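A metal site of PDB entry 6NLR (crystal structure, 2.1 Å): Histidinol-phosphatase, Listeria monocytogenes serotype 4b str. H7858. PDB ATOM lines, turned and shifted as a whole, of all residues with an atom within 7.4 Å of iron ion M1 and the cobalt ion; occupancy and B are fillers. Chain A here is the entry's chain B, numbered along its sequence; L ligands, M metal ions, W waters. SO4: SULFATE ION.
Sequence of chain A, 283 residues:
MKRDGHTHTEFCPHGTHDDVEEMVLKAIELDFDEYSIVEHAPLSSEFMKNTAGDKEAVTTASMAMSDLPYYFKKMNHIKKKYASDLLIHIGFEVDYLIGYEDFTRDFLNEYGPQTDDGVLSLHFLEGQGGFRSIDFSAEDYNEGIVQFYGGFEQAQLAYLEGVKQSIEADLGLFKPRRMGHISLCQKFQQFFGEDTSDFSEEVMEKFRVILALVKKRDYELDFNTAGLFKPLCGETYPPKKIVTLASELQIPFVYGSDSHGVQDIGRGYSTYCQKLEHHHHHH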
ATOM      1  N   HIS A   6     -28.416  10.937 -24.726  1.00  0.00           N
ATOM      2  CA  HIS A   6     -28.648  10.495 -23.317  1.00  0.00           C
ATOM      3  C   HIS A   6     -29.695   9.364 -23.235  1.00  0.00           C
ATOM      4  O   HIS A   6     -30.915   9.654 -23.160  1.00  0.00           O
ATOM      5  CB  HIS A   6     -28.992  11.732 -22.477  1.00  0.00           C
ATOM      6  CG  HIS A   6     -28.946  11.522 -20.993  1.00  0.00           C
ATOM      7  ND1 HIS A   6     -28.784  12.569 -20.113  1.00  0.00           N
ATOM      8  CD2 HIS A   6     -29.020  10.398 -20.241  1.00  0.00           C
ATOM      9  CE1 HIS A   6     -28.790  12.101 -18.880  1.00  0.00           C
ATOM     10  NE2 HIS A   6     -28.932  10.767 -18.922  1.00  0.00           N
ATOM     11  N   THR A   7     -29.237   8.114 -23.210  1.00  0.00           N
ATOM     12  CA  THR A   7     -30.107   6.924 -23.083  1.00  0.00           C
ATOM     13  C   THR A   7     -29.474   5.912 -22.123  1.00  0.00           C
ATOM     14  O   THR A   7     -28.227   5.904 -21.961  1.00  0.00           O
ATOM     15  CB  THR A   7     -30.407   6.256 -24.425  1.00  0.00           C
ATOM     16  OG1 THR A   7     -29.234   5.552 -24.870  1.00  0.00           O
ATOM     17  CG2 THR A   7     -30.889   7.253 -25.452  1.00  0.00           C
ATOM     18  N   HIS A   8     -30.336   5.070 -21.568  1.00  0.00           N
ATOM     19  CA  HIS A   8     -30.004   4.011 -20.590  1.00  0.00           C
ATOM     20  C   HIS A   8     -30.435   2.656 -21.157  1.00  0.00           C
ATOM     21  O   HIS A   8     -30.991   2.621 -22.259  1.00  0.00           O
ATOM     22  CB  HIS A   8     -30.622   4.375 -19.240  1.00  0.00           C
ATOM     23  CG  HIS A   8     -30.022   5.625 -18.673  1.00  0.00           C
ATOM     24  ND1 HIS A   8     -28.869   5.591 -17.942  1.00  0.00           N
ATOM     25  CD2 HIS A   8     -30.395   6.920 -18.749  1.00  0.00           C
ATOM     26  CE1 HIS A   8     -28.562   6.821 -17.562  1.00  0.00           C
ATOM     27  NE2 HIS A   8     -29.471   7.656 -18.060  1.00  0.00           N
ATOM     28  N   HIS A  14     -32.758   0.737 -11.970  1.00  0.00           N
ATOM     29  CA  HIS A  14     -34.025   1.492 -11.752  1.00  0.00           C
ATOM     30  C   HIS A  14     -34.773   1.746 -13.064  1.00  0.00           C
ATOM     31  O   HIS A  14     -35.776   2.470 -13.020  1.00  0.00           O
ATOM     32  CB  HIS A  14     -33.755   2.811 -11.003  1.00  0.00           C
ATOM     33  CG  HIS A  14     -32.795   3.732 -11.685  1.00  0.00           C
ATOM     34  ND1 HIS A  14     -31.444   3.773 -11.363  1.00  0.00           N
ATOM     35  CD2 HIS A  14     -32.977   4.661 -12.661  1.00  0.00           C
ATOM     36  CE1 HIS A  14     -30.843   4.680 -12.105  1.00  0.00           C
ATOM     37  NE2 HIS A  14     -31.760   5.231 -12.906  1.00  0.00           N
ATOM     38  N   VAL A  38     -25.346   5.895 -22.507  1.00  0.00           N
ATOM     39  CA  VAL A  38     -24.558   6.496 -21.390  1.00  0.00           C
ATOM     40  C   VAL A  38     -25.146   5.966 -20.088  1.00  0.00           C
ATOM     41  O   VAL A  38     -25.830   6.683 -19.369  1.00  0.00           O
ATOM     42  CB  VAL A  38     -24.474   8.023 -21.502  1.00  0.00           C
ATOM     43  CG1 VAL A  38     -23.494   8.418 -22.599  1.00  0.00           C
ATOM     44  CG2 VAL A  38     -25.831   8.656 -21.763  1.00  0.00           C
ATOM     45  N   GLU A  39     -24.885   4.690 -19.824  1.00  0.00           N
ATOM     46  CA  GLU A  39     -25.402   4.007 -18.615  1.00  0.00           C
ATOM     47  C   GLU A  39     -24.751   4.621 -17.369  1.00  0.00           C
ATOM     48  O   GLU A  39     -23.604   5.106 -17.434  1.00  0.00           O
ATOM     49  CB  GLU A  39     -25.167   2.505 -18.721  1.00  0.00           C
ATOM     50  CG  GLU A  39     -25.946   1.744 -17.674  1.00  0.00           C
ATOM     51  CD  GLU A  39     -27.418   2.149 -17.660  1.00  0.00           C
ATOM     52  OE1 GLU A  39     -28.155   1.621 -18.514  1.00  0.00           O
ATOM     53  OE2 GLU A  39     -27.790   3.051 -16.864  1.00  0.00           O
ATOM     54  N   HIS A  40     -25.472   4.626 -16.252  1.00  0.00           N
ATOM     55  CA  HIS A  40     -24.916   5.090 -14.948  1.00  0.00           C
ATOM     56  C   HIS A  40     -23.629   4.337 -14.608  1.00  0.00           C
ATOM     57  O   HIS A  40     -23.674   3.083 -14.558  1.00  0.00           O
ATOM     58  CB  HIS A  40     -25.927   4.872 -13.850  1.00  0.00           C
ATOM     59  CG  HIS A  40     -27.147   5.681 -14.054  1.00  0.00           C
ATOM     60  ND1 HIS A  40     -27.138   7.046 -13.845  1.00  0.00           N
ATOM     61  CD2 HIS A  40     -28.388   5.335 -14.432  1.00  0.00           C
ATOM     62  CE1 HIS A  40     -28.345   7.525 -14.088  1.00  0.00           C
ATOM     63  NE2 HIS A  40     -29.121   6.484 -14.446  1.00  0.00           N
ATOM     64  N   GLU A  93     -23.130   7.884 -18.078  1.00  0.00           N
ATOM     65  CA  GLU A  93     -23.570   9.010 -17.248  1.00  0.00           C
ATOM     66  C   GLU A  93     -22.784   8.871 -15.943  1.00  0.00           C
ATOM     67  O   GLU A  93     -23.082   7.959 -15.143  1.00  0.00           O
ATOM     68  CB  GLU A  93     -25.075   9.037 -17.035  1.00  0.00           C
ATOM     69  CG  GLU A  93     -25.508  10.342 -16.385  1.00  0.00           C
ATOM     70  CD  GLU A  93     -26.980  10.440 -16.039  1.00  0.00           C
ATOM     71  OE1 GLU A  93     -27.707   9.495 -16.356  1.00  0.00           O
ATOM     72  OE2 GLU A  93     -27.394  11.483 -15.479  1.00  0.00           O
ATOM     73  N   ASP A  95     -21.555  10.113 -12.382  1.00  0.00           N
ATOM     74  CA  ASP A  95     -21.863  10.951 -11.198  1.00  0.00           C
ATOM     75  C   ASP A  95     -20.649  11.828 -10.886  1.00  0.00           C
ATOM     76  O   ASP A  95     -19.524  11.313 -10.798  1.00  0.00           O
ATOM     77  CB  ASP A  95     -22.243  10.110  -9.989  1.00  0.00           C
ATOM     78  CG  ASP A  95     -23.699   9.703 -10.016  1.00  0.00           C
ATOM     79  OD1 ASP A  95     -24.526  10.482  -9.531  1.00  0.00           O
ATOM     80  OD2 ASP A  95     -23.979   8.654 -10.584  1.00  0.00           O
ATOM     81  N   VAL A 119     -21.670  11.855 -20.280  1.00  0.00           N
ATOM     82  CA  VAL A 119     -22.393  12.953 -19.598  1.00  0.00           C
ATOM     83  C   VAL A 119     -21.902  12.971 -18.146  1.00  0.00           C
ATOM     84  O   VAL A 119     -21.771  11.882 -17.542  1.00  0.00           O
ATOM     85  CB  VAL A 119     -23.902  12.729 -19.703  1.00  0.00           C
ATOM     86  CG1 VAL A 119     -24.688  13.743 -18.889  1.00  0.00           C
ATOM     87  CG2 VAL A 119     -24.370  12.724 -21.163  1.00  0.00           C
ATOM     88  N   SER A 121     -23.004  14.240 -14.522  1.00  0.00           N
ATOM     89  CA  SER A 121     -24.290  14.544 -13.856  1.00  0.00           C
ATOM     90  C   SER A 121     -24.114  14.637 -12.343  1.00  0.00           C
ATOM     91  O   SER A 121     -23.447  13.779 -11.767  1.00  0.00           O
ATOM     92  CB  SER A 121     -25.320  13.515 -14.214  1.00  0.00           C
ATOM     93  OG  SER A 121     -25.702  13.659 -15.565  1.00  0.00           O
ATOM     94  N   LEU A 122     -24.730  15.642 -11.730  1.00  0.00           N
ATOM     95  CA  LEU A 122     -24.869  15.743 -10.256  1.00  0.00           C
ATOM     96  C   LEU A 122     -26.230  15.173  -9.824  1.00  0.00           C
ATOM     97  O   LEU A 122     -27.265  15.725 -10.233  1.00  0.00           O
ATOM     98  CB  LEU A 122     -24.699  17.206  -9.863  1.00  0.00           C
ATOM     99  CG  LEU A 122     -24.689  17.471  -8.366  1.00  0.00           C
ATOM    100  CD1 LEU A 122     -23.442  16.911  -7.704  1.00  0.00           C
ATOM    101  CD2 LEU A 122     -24.787  18.955  -8.124  1.00  0.00           C
ATOM    102  N   HIS A 123     -26.223  14.125  -8.984  1.00  0.00           N
ATOM    103  CA  HIS A 123     -27.464  13.432  -8.499  1.00  0.00           C
ATOM    104  C   HIS A 123     -27.542  13.437  -6.968  1.00  0.00           C
ATOM    105  O   HIS A 123     -28.634  13.145  -6.444  1.00  0.00           O
ATOM    106  CB  HIS A 123     -27.565  11.982  -8.990  1.00  0.00           C
ATOM    107  CG  HIS A 123     -27.634  11.817 -10.463  1.00  0.00           C
ATOM    108  ND1 HIS A 123     -26.704  11.078 -11.147  1.00  0.00           N
ATOM    109  CD2 HIS A 123     -28.514  12.265 -11.384  1.00  0.00           C
ATOM    110  CE1 HIS A 123     -27.002  11.093 -12.441  1.00  0.00           C
ATOM    111  NE2 HIS A 123     -28.085  11.827 -12.596  1.00  0.00           N
ATOM    112  N   ASP A 135     -33.070  13.470  -6.841  1.00  0.00           N
ATOM    113  CA  ASP A 135     -34.102  13.119  -7.866  1.00  0.00           C
ATOM    114  C   ASP A 135     -34.869  11.841  -7.516  1.00  0.00           C
ATOM    115  O   ASP A 135     -35.608  11.380  -8.371  1.00  0.00           O
ATOM    116  CB  ASP A 135     -33.473  13.029  -9.265  1.00  0.00           C
ATOM    117  CG  ASP A 135     -32.437  11.942  -9.437  1.00  0.00           C
ATOM    118  OD1 ASP A 135     -31.994  11.366  -8.411  1.00  0.00           O
ATOM    119  OD2 ASP A 135     -32.060  11.685 -10.603  1.00  0.00           O
ATOM    120  N   GLY A 180     -24.823  17.055 -17.603  1.00  0.00           N
ATOM    121  CA  GLY A 180     -26.153  16.479 -17.581  1.00  0.00           C
ATOM    122  C   GLY A 180     -27.183  17.358 -16.885  1.00  0.00           C
ATOM    123  O   GLY A 180     -26.861  17.960 -15.852  1.00  0.00           O
ATOM    124  N   HIS A 181     -28.392  17.432 -17.450  1.00  0.00           N
ATOM    125  CA  HIS A 181     -29.612  18.045 -16.883  1.00  0.00           C
ATOM    126  C   HIS A 181     -29.296  19.069 -15.773  1.00  0.00           C
ATOM    127  O   HIS A 181     -29.623  18.780 -14.616  1.00  0.00           O
ATOM    128  CB  HIS A 181     -30.580  16.931 -16.418  1.00  0.00           C
ATOM    129  CG  HIS A 181     -29.952  15.819 -15.648  1.00  0.00           C
ATOM    130  ND1 HIS A 181     -29.141  16.048 -14.530  1.00  0.00           N
ATOM    131  CD2 HIS A 181     -30.018  14.485 -15.808  1.00  0.00           C
ATOM    132  CE1 HIS A 181     -28.749  14.879 -14.032  1.00  0.00           C
ATOM    133  NE2 HIS A 181     -29.282  13.893 -14.792  1.00  0.00           N
ATOM    134  N   LEU A 184     -31.652  19.991 -12.348  1.00  0.00           N
ATOM    135  CA  LEU A 184     -32.299  18.780 -11.759  1.00  0.00           C
ATOM    136  C   LEU A 184     -32.949  19.138 -10.417  1.00  0.00           C
ATOM    137  O   LEU A 184     -33.859  18.394  -9.982  1.00  0.00           O
ATOM    138  CB  LEU A 184     -31.278  17.658 -11.611  1.00  0.00           C
ATOM    139  CG  LEU A 184     -31.905  16.289 -11.277  1.00  0.00           C
ATOM    140  CD1 LEU A 184     -32.720  15.717 -12.454  1.00  0.00           C
ATOM    141  CD2 LEU A 184     -30.823  15.309 -10.850  1.00  0.00           C
ATOM    142  N   ASP A 222     -26.412  18.932 -22.057  1.00  0.00           N
ATOM    143  CA  ASP A 222     -27.550  17.970 -22.190  1.00  0.00           C
ATOM    144  C   ASP A 222     -28.850  18.791 -22.271  1.00  0.00           C
ATOM    145  O   ASP A 222     -29.163  19.442 -21.281  1.00  0.00           O
ATOM    146  CB  ASP A 222     -27.479  17.044 -20.975  1.00  0.00           C
ATOM    147  CG  ASP A 222     -28.480  15.910 -20.835  1.00  0.00           C
ATOM    148  OD1 ASP A 222     -28.833  15.287 -21.849  1.00  0.00           O
ATOM    149  OD2 ASP A 222     -28.856  15.630 -19.663  1.00  0.00           O
ATOM    150  N   ASN A 224     -32.233  18.182 -21.912  1.00  0.00           N
ATOM    151  CA  ASN A 224     -32.839  16.944 -21.340  1.00  0.00           C
ATOM    152  C   ASN A 224     -34.368  17.122 -21.219  1.00  0.00           C
ATOM    153  O   ASN A 224     -34.813  17.995 -20.465  1.00  0.00           O
ATOM    154  CB  ASN A 224     -32.114  16.581 -20.039  1.00  0.00           C
ATOM    155  CG  ASN A 224     -32.522  15.225 -19.473  1.00  0.00           C
ATOM    156  OD1 ASN A 224     -33.717  14.893 -19.419  1.00  0.00           O
ATOM    157  ND2 ASN A 224     -31.533  14.452 -19.064  1.00  0.00           N
ATOM    158  N   SER A 257     -33.081  12.357 -24.350  1.00  0.00           N
ATOM    159  CA  SER A 257     -34.373  11.790 -23.928  1.00  0.00           C
ATOM    160  C   SER A 257     -34.294  11.297 -22.478  1.00  0.00           C
ATOM    161  O   SER A 257     -35.333  11.210 -21.811  1.00  0.00           O
ATOM    162  CB  SER A 257     -34.767  10.672 -24.843  1.00  0.00           C
ATOM    163  OG  SER A 257     -33.846   9.600 -24.770  1.00  0.00           O
ATOM    164  N   ASP A 258     -33.102  10.955 -22.000  1.00  0.00           N
ATOM    165  CA  ASP A 258     -32.911  10.232 -20.711  1.00  0.00           C
ATOM    166  C   ASP A 258     -33.769   8.963 -20.719  1.00  0.00           C
ATOM    167  O   ASP A 258     -34.359   8.635 -19.687  1.00  0.00           O
ATOM    168  CB  ASP A 258     -33.213  11.142 -19.519  1.00  0.00           C
ATOM    169  CG  ASP A 258     -32.220  10.965 -18.396  1.00  0.00           C
ATOM    170  OD1 ASP A 258     -31.625   9.867 -18.299  1.00  0.00           O
ATOM    171  OD2 ASP A 258     -31.986  11.953 -17.685  1.00  0.00           O
ATOM    172  N   SER A 259     -33.833   8.259 -21.852  1.00  0.00           N
ATOM    173  CA  SER A 259     -34.719   7.098 -22.055  1.00  0.00           C
ATOM    174  C   SER A 259     -34.289   5.938 -21.156  1.00  0.00           C
ATOM    175  O   SER A 259     -33.091   5.596 -21.155  1.00  0.00           O
ATOM    176  CB  SER A 259     -34.759   6.689 -23.513  1.00  0.00           C
ATOM    177  OG  SER A 259     -35.495   7.640 -24.281  1.00  0.00           O
ATOM    178  N   HIS A 260     -35.226   5.383 -20.396  1.00  0.00           N
ATOM    179  CA  HIS A 260     -35.028   4.175 -19.548  1.00  0.00           C
ATOM    180  C   HIS A 260     -35.829   2.989 -20.101  1.00  0.00           C
ATOM    181  O   HIS A 260     -35.861   1.923 -19.456  1.00  0.00           O
ATOM    182  CB  HIS A 260     -35.367   4.508 -18.101  1.00  0.00           C
ATOM    183  CG  HIS A 260     -34.344   5.395 -17.484  1.00  0.00           C
ATOM    184  ND1 HIS A 260     -33.407   4.925 -16.598  1.00  0.00           N
ATOM    185  CD2 HIS A 260     -34.090   6.712 -17.652  1.00  0.00           C
ATOM    186  CE1 HIS A 260     -32.650   5.927 -16.207  1.00  0.00           C
ATOM    187  NE2 HIS A 260     -33.060   7.039 -16.819  1.00  0.00           N
HETATM  188  S   SO4 L   1     -31.328   9.343 -14.481  1.00  0.00           S
HETATM  189  O1  SO4 L   1     -30.324  10.135 -13.815  1.00  0.00           O
HETATM  190  O2  SO4 L   1     -32.523  10.131 -14.692  1.00  0.00           O
HETATM  191  O3  SO4 L   1     -30.802   8.892 -15.768  1.00  0.00           O
HETATM  192  O4  SO4 L   1     -31.654   8.202 -13.669  1.00  0.00           O
HETATM  193 FE    FE M   1     -29.141  11.733 -14.466  1.00  0.00          FE
HETATM  194 CO    CO M   2     -29.685   9.627 -17.254  1.00  0.00          CO
HETATM  195 FE    FE M   3     -31.270   6.508 -14.485  1.00  0.00          FE
HETATM  196  O   HOH W   1     -31.074  12.178 -13.394  1.00  0.00           O
HETATM  197  O   HOH W   2     -30.138  11.331 -16.355  1.00  0.00           O
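Iron ion M1 is bound by the side-chain carboxylate of Glu 93, an oxygen (O1) of the ligand, a ring nitrogen (NE2) of His 123, water W2, a ring nitrogen (NE2) of His 181 and water W1. Iron ion M1 has six donor atoms within binding distance.
The backbone carbonyl oxygen (O) of Val 38 sits at hydrogen-bond distance from the backbone NH (N) of Glu 93 (3.2 Å). The side-chain carboxylate of Glu 39 lies within hydrogen-bond range of a ring nitrogen (ND1) of His 8, at 3.0 Å. ND2 of Asn 224 is in hydrogen-bond range of ND1 of His 6. N of Ser 259 is in hydrogen-bond range of O of His 6 (3.5 Å). A ring nitrogen (ND1) of His 6 is in hydrogen-bond range of the side-chain carboxylate of Asp 222 (3.1 Å). The side-chain hydroxyl (OG) of Ser 257 sits at hydrogen-bond distance from the backbone carbonyl oxygen (O) of His 6 (3.3 Å). The side-chain carboxylate of Asp 222 sits at hydrogen-bond distance from the backbone NH of His 181, 2.9 Å away. NE2 of His 260 sits close to OD1 of Asp 258, 3.5 Å away.
Along chain A the residues within 4 Å of iron ion M1 span positions 93 to 181.
Water W2 is bound to the cobalt ion (2.0 Å). An oxygen (O3) of the ligand is bound to the cobalt ion, 2.0 Å away. NE2 of His 8 is bound to the cobalt ion, 2.1 Å away. NE2 of His 6 is bound to the cobalt ion, at 2.2 Å. The cobalt ion is bound by OE1 of Glu 93 (2.2 Å). OD1 of Asp 258 is bound to the cobalt ion (2.2 Å). The cobalt ion has six donor atoms within binding distance.
The nearest printed residue that does not touch the cobalt ion is His 40 (4.03 Å).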
